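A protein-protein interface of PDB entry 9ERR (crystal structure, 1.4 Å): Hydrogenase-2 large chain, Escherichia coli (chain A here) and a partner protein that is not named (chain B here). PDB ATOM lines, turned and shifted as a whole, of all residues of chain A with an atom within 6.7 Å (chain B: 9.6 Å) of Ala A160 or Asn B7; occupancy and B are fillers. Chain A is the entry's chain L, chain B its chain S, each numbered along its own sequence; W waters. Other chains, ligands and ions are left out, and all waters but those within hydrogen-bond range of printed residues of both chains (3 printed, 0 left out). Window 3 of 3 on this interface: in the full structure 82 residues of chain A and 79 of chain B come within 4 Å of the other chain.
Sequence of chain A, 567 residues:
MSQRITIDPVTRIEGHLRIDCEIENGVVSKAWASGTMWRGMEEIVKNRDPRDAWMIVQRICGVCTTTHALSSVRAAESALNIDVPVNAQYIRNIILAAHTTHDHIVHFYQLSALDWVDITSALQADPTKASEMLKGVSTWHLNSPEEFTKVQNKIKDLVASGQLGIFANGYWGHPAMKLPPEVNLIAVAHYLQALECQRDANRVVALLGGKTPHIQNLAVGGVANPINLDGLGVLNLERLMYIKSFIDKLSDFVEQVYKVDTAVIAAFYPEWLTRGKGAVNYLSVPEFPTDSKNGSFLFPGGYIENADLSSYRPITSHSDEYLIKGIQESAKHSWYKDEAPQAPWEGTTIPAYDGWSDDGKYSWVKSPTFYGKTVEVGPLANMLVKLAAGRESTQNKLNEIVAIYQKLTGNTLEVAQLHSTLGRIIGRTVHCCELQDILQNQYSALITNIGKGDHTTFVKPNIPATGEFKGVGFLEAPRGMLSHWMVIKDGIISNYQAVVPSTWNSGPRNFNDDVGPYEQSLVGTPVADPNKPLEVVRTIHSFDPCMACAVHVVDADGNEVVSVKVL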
ATOM      1  N   ILE A 155     -19.857 -22.608   0.509  1.00  0.00           N
ATOM      2  CA  ILE A 155     -20.575 -23.003   1.708  1.00  0.00           C
ATOM      3  C   ILE A 155     -21.237 -24.373   1.482  1.00  0.00           C
ATOM      4  O   ILE A 155     -21.279 -25.201   2.376  1.00  0.00           O
ATOM      5  CB  ILE A 155     -21.672 -22.005   2.099  1.00  0.00           C
ATOM      6  CG1 ILE A 155     -21.219 -20.548   2.204  1.00  0.00           C
ATOM      7  CG2 ILE A 155     -22.312 -22.460   3.407  1.00  0.00           C
ATOM      8  CD1 ILE A 155     -22.413 -19.603   2.203  1.00  0.00           C
ATOM      9  N   LYS A 156     -21.890 -24.541   0.335  1.00  0.00           N
ATOM     10  CA  LYS A 156     -22.557 -25.789   0.001  1.00  0.00           C
ATOM     11  C   LYS A 156     -21.590 -26.967   0.167  1.00  0.00           C
ATOM     12  O   LYS A 156     -21.943 -27.949   0.829  1.00  0.00           O
ATOM     13  CB  LYS A 156     -23.084 -25.750  -1.435  1.00  0.00           C
ATOM     14  CG  LYS A 156     -23.955 -26.934  -1.848  1.00  0.00           C
ATOM     15  CD  LYS A 156     -24.653 -26.754  -3.199  1.00  0.00           C
ATOM     16  CE  LYS A 156     -25.080 -25.319  -3.452  1.00  0.00           C
ATOM     17  NZ  LYS A 156     -26.129 -25.191  -4.503  1.00  0.00           N
ATOM     18  N   ASP A 157     -20.396 -26.845  -0.414  1.00  0.00           N
ATOM     19  CA  ASP A 157     -19.371 -27.874  -0.355  1.00  0.00           C
ATOM     20  C   ASP A 157     -18.952 -28.163   1.083  1.00  0.00           C
ATOM     21  O   ASP A 157     -18.786 -29.318   1.483  1.00  0.00           O
ATOM     22  CB  ASP A 157     -18.170 -27.521  -1.235  1.00  0.00           C
ATOM     23  CG  ASP A 157     -18.426 -27.561  -2.733  1.00  0.00           C
ATOM     24  OD1 ASP A 157     -19.478 -28.038  -3.135  1.00  0.00           O
ATOM     25  OD2 ASP A 157     -17.599 -27.052  -3.443  1.00  0.00           O
ATOM     26  N   LEU A 158     -18.754 -27.106   1.884  1.00  0.00           N
ATOM     27  CA  LEU A 158     -18.392 -27.310   3.271  1.00  0.00           C
ATOM     28  C   LEU A 158     -19.513 -28.063   3.993  1.00  0.00           C
ATOM     29  O   LEU A 158     -19.234 -29.006   4.707  1.00  0.00           O
ATOM     30  CB  LEU A 158     -18.129 -25.946   3.920  1.00  0.00           C
ATOM     31  CG  LEU A 158     -17.796 -26.027   5.406  1.00  0.00           C
ATOM     32  CD1 LEU A 158     -16.296 -25.912   5.631  1.00  0.00           C
ATOM     33  CD2 LEU A 158     -18.562 -24.965   6.160  1.00  0.00           C
ATOM     34  N   VAL A 159     -20.777 -27.641   3.862  1.00  0.00           N
ATOM     35  CA  VAL A 159     -21.875 -28.299   4.569  1.00  0.00           C
ATOM     36  C   VAL A 159     -21.971 -29.757   4.121  1.00  0.00           C
ATOM     37  O   VAL A 159     -22.112 -30.664   4.962  1.00  0.00           O
ATOM     38  CB  VAL A 159     -23.204 -27.543   4.372  1.00  0.00           C
ATOM     39  CG1 VAL A 159     -24.437 -28.328   4.858  1.00  0.00           C
ATOM     40  CG2 VAL A 159     -23.147 -26.171   5.041  1.00  0.00           C
ATOM     41  N   ALA A 160     -21.797 -29.978   2.817  1.00  0.00           N
ATOM     42  CA  ALA A 160     -21.915 -31.309   2.242  1.00  0.00           C
ATOM     43  C   ALA A 160     -20.842 -32.254   2.785  1.00  0.00           C
ATOM     44  O   ALA A 160     -21.098 -33.448   2.900  1.00  0.00           O
ATOM     45  CB  ALA A 160     -21.832 -31.247   0.743  1.00  0.00           C
ATOM     46  N   SER A 161     -19.649 -31.732   3.102  1.00  0.00           N
ATOM     47  CA  SER A 161     -18.547 -32.538   3.603  1.00  0.00           C
ATOM     48  C   SER A 161     -18.874 -33.165   4.951  1.00  0.00           C
ATOM     49  O   SER A 161     -18.192 -34.081   5.395  1.00  0.00           O
ATOM     50  CB  SER A 161     -17.271 -31.733   3.701  1.00  0.00           C
ATOM     51  OG  SER A 161     -17.243 -30.919   4.875  1.00  0.00           O
ATOM     52  N   GLY A 162     -19.835 -32.599   5.667  1.00  0.00           N
ATOM     53  CA  GLY A 162     -20.132 -33.016   7.028  1.00  0.00           C
ATOM     54  C   GLY A 162     -19.080 -32.547   8.032  1.00  0.00           C
ATOM     55  O   GLY A 162     -19.168 -32.920   9.193  1.00  0.00           O
ATOM     56  N   GLN A 163     -18.114 -31.727   7.591  1.00  0.00           N
ATOM     57  CA  GLN A 163     -17.082 -31.169   8.458  1.00  0.00           C
ATOM     58  C   GLN A 163     -17.241 -29.654   8.503  1.00  0.00           C
ATOM     59  O   GLN A 163     -16.650 -28.950   7.689  1.00  0.00           O
ATOM     60  CB  GLN A 163     -15.697 -31.500   7.915  1.00  0.00           C
ATOM     61  CG  GLN A 163     -15.384 -32.977   7.943  1.00  0.00           C
ATOM     62  CD  GLN A 163     -13.958 -33.215   7.513  1.00  0.00           C
ATOM     63  OE1 GLN A 163     -13.612 -33.008   6.354  1.00  0.00           O
ATOM     64  NE2 GLN A 163     -13.136 -33.631   8.462  1.00  0.00           N
ATOM     65  N   LEU A 164     -18.119 -29.182   9.399  1.00  0.00           N
ATOM     66  CA  LEU A 164     -18.485 -27.776   9.428  1.00  0.00           C
ATOM     67  C   LEU A 164     -17.436 -26.933  10.164  1.00  0.00           C
ATOM     68  O   LEU A 164     -17.406 -25.712   9.932  1.00  0.00           O
ATOM     69  CB  LEU A 164     -19.847 -27.586  10.101  1.00  0.00           C
ATOM     70  CG  LEU A 164     -21.086 -27.692   9.209  1.00  0.00           C
ATOM     71  CD1 LEU A 164     -21.081 -26.629   8.163  1.00  0.00           C
ATOM     72  CD2 LEU A 164     -21.184 -29.071   8.584  1.00  0.00           C
ATOM     73  N   ASN B   7     -14.680 -33.177  -3.378  1.00  0.00           N
ATOM     74  CA  ASN B   7     -14.987 -32.627  -2.022  1.00  0.00           C
ATOM     75  C   ASN B   7     -14.574 -33.644  -0.943  1.00  0.00           C
ATOM     76  O   ASN B   7     -15.411 -34.126  -0.177  1.00  0.00           O
ATOM     77  CB  ASN B   7     -16.458 -32.170  -1.950  1.00  0.00           C
ATOM     78  CG  ASN B   7     -16.794 -31.305  -0.742  1.00  0.00           C
ATOM     79  OD1 ASN B   7     -15.958 -30.533  -0.284  1.00  0.00           O
ATOM     80  ND2 ASN B   7     -18.008 -31.424  -0.212  1.00  0.00           N
ATOM     81  N   PRO B   8     -13.263 -33.971  -0.786  1.00  0.00           N
ATOM     82  CA  PRO B   8     -12.830 -35.006   0.173  1.00  0.00           C
ATOM     83  C   PRO B   8     -12.939 -34.583   1.646  1.00  0.00           C
ATOM     84  O   PRO B   8     -13.198 -33.407   1.957  1.00  0.00           O
ATOM     85  CB  PRO B   8     -11.350 -35.214  -0.212  1.00  0.00           C
ATOM     86  CG  PRO B   8     -10.906 -33.842  -0.720  1.00  0.00           C
ATOM     87  CD  PRO B   8     -12.125 -33.309  -1.457  1.00  0.00           C
ATOM     88  N   GLN B   9     -12.683 -35.526   2.563  1.00  0.00           N
ATOM     89  CA  GLN B   9     -12.575 -35.189   3.979  1.00  0.00           C
ATOM     90  C   GLN B   9     -11.232 -34.506   4.248  1.00  0.00           C
ATOM     91  O   GLN B   9     -10.252 -34.840   3.605  1.00  0.00           O
ATOM     92  CB  GLN B   9     -12.701 -36.427   4.849  1.00  0.00           C
ATOM     93  CG  GLN B   9     -14.077 -37.071   4.710  1.00  0.00           C
ATOM     94  CD  GLN B   9     -15.150 -36.232   5.348  1.00  0.00           C
ATOM     95  OE1 GLN B   9     -15.183 -36.047   6.564  1.00  0.00           O
ATOM     96  NE2 GLN B   9     -16.028 -35.693   4.520  1.00  0.00           N
ATOM     97  N   ARG B  10     -11.199 -33.580   5.219  1.00  0.00           N
ATOM     98  CA  ARG B  10     -10.004 -32.804   5.521  1.00  0.00           C
ATOM     99  C   ARG B  10      -9.477 -33.208   6.886  1.00  0.00           C
ATOM    100  O   ARG B  10     -10.248 -33.527   7.795  1.00  0.00           O
ATOM    101  CB  ARG B  10     -10.324 -31.301   5.510  1.00  0.00           C
ATOM    102  CG  ARG B  10     -10.561 -30.743   4.108  1.00  0.00           C
ATOM    103  CD  ARG B  10     -11.282 -29.410   4.095  1.00  0.00           C
ATOM    104  NE  ARG B  10     -12.725 -29.525   4.313  1.00  0.00           N
ATOM    105  CZ  ARG B  10     -13.418 -28.976   5.286  1.00  0.00           C
ATOM    106  NH1 ARG B  10     -12.834 -28.136   6.131  1.00  0.00           N
ATOM    107  NH2 ARG B  10     -14.716 -29.235   5.374  1.00  0.00           N
ATOM    108  N   LEU B  41     -11.113 -23.852   4.831  1.00  0.00           N
ATOM    109  CA  LEU B  41     -12.082 -24.419   3.888  1.00  0.00           C
ATOM    110  C   LEU B  41     -11.479 -25.563   3.078  1.00  0.00           C
ATOM    111  O   LEU B  41     -12.246 -26.417   2.616  1.00  0.00           O
ATOM    112  CB  LEU B  41     -12.635 -23.358   2.938  1.00  0.00           C
ATOM    113  CG  LEU B  41     -13.382 -22.203   3.596  1.00  0.00           C
ATOM    114  CD1 LEU B  41     -13.827 -21.227   2.535  1.00  0.00           C
ATOM    115  CD2 LEU B  41     -14.561 -22.699   4.421  1.00  0.00           C
ATOM    116  N   GLU B  42     -10.146 -25.577   2.885  1.00  0.00           N
ATOM    117  CA  GLU B  42      -9.509 -26.523   1.959  1.00  0.00           C
ATOM    118  C   GLU B  42      -8.492 -27.440   2.641  1.00  0.00           C
ATOM    119  O   GLU B  42      -8.480 -28.636   2.373  1.00  0.00           O
ATOM    120  CB  GLU B  42      -8.777 -25.810   0.815  1.00  0.00           C
ATOM    121  CG  GLU B  42      -9.696 -25.088  -0.157  1.00  0.00           C
ATOM    122  CD  GLU B  42      -9.021 -24.265  -1.247  1.00  0.00           C
ATOM    123  OE1 GLU B  42      -7.781 -24.234  -1.295  1.00  0.00           O
ATOM    124  OE2 GLU B  42      -9.744 -23.600  -2.000  1.00  0.00           O
ATOM    125  N   LYS B  70     -14.979 -38.337  17.548  1.00  0.00           N
ATOM    126  CA  LYS B  70     -15.054 -38.685  16.133  1.00  0.00           C
ATOM    127  C   LYS B  70     -13.654 -38.880  15.541  1.00  0.00           C
ATOM    128  O   LYS B  70     -13.425 -39.803  14.741  1.00  0.00           O
ATOM    129  CB  LYS B  70     -15.863 -37.636  15.357  1.00  0.00           C
ATOM    130  CG  LYS B  70     -15.935 -37.768  13.837  1.00  0.00           C
ATOM    131  CD  LYS B  70     -16.827 -36.722  13.161  1.00  0.00           C
ATOM    132  CE  LYS B  70     -16.912 -36.836  11.655  1.00  0.00           C
ATOM    133  NZ  LYS B  70     -17.658 -35.707  11.015  1.00  0.00           N
HETATM  134  O   HOH W   1     -17.354 -36.010   8.175  1.00  0.00           O
HETATM  135  O   HOH W   2     -14.216 -31.881   3.706  1.00  0.00           O
HETATM  136  O   HOH W   3     -14.433 -27.687   8.514  1.00  0.00           O
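Ile A155 touches none of the printed residues of chain B.
Asp A157 touches just one residue of chain B: Asn B7 (2.8 Å).
Val A159 touches none of the printed residues of chain B.
Ala A160 touches just one residue of chain B: Asn B7.
Of the printed residues of chain B, Gly A162 touches Lys B70.
Asn B7 touches just these residues of chain A: Asp A157 (2.8 Å), Ala A160 (3.9 Å) and Ser A161 (3.7 Å).
Printed residues of chain A within 4 Å of Gln B9: Ser A161 (2.8 Å) and Gln A163 (3.2 Å).
Of the printed residues of chain A, Arg B10 touches Leu A158 (3.7 Å), Ser A161 (3.1 Å) and Gln A163 (2.7 Å).
Of the printed residues of chain A, Leu B41 touches Leu A158.
Of the printed residues of chain A, Lys B70 touches Gly A162 (3.7 Å).
The nearest residue of chain B that does not touch Ala A160 is Gln B9 (5.8 Å).
The side-chain amide nitrogen (ND2) of Asn B7 sits at hydrogen-bond distance from the backbone carbonyl oxygen (O) of Asp A157, 2.8 Å away.
The side-chain amide nitrogen (NE2) of Gln B9 sits at hydrogen-bond distance from the backbone carbonyl oxygen (O) of Ser A161, 2.8 Å away.
OE1 of Gln B9 sits close to OE1 of Gln A163 (3.4 Å).
The guanidinium group (NH2) of Arg B10 is in hydrogen-bond range of the side-chain hydroxyl (OG) of Ser A161.
N of Arg B10 is in hydrogen-bond range of OE1 of Gln A163, 2.7 Å away.
The side-chain hydroxyl (OG) of Ser A161 sits at hydrogen-bond distance from the backbone carbonyl oxygen (O) of Leu A158 (2.8 Å).
The side-chain hydroxyl of Ser A161 is in hydrogen-bond range of the backbone NH of Gln A163 (3.0 Å).
Among the printed residues, pairs that only touch across the chains: Gly A162 with Lys B70 (3.7 Å), Leu A158 with Arg B10 (3.7 Å), Ser A161 with Asn B7 (3.7 Å), Leu A158 with Leu B41 (3.8 Å) and Ala A160 with Asn B7 (3.9 Å).
Water W2 lies within hydrogen-bond range of the backbone carbonyl oxygen (O) of Pro B8 (2.5 Å), the guanidinium group (NE) of Arg B10 (2.9 Å), the side-chain amide oxygen (OE1) of Gln A163 (2.9 Å) and the side-chain hydroxyl (OG) of Ser A161 (3.4 Å).
Water W3 lies within hydrogen-bond range of the backbone carbonyl oxygen (O) of Gln A163 and the guanidinium group (NH1) of Arg B10.
Water W1 lies within hydrogen-bond range of OE1 of Gln B9 (2.7 Å), NZ of Lys B70 (2.9 Å) and O of Ser A161 (3.5 Å).
Printed residues of chain B that touch a printed residue of chain A: Asn B7, Gln B9, Arg B10, Leu B41 and Lys B70.
Hydrophobic or aromatic side chains of chain A within 4 Å of the printed part of chain B: Leu A158 and Ala A160.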
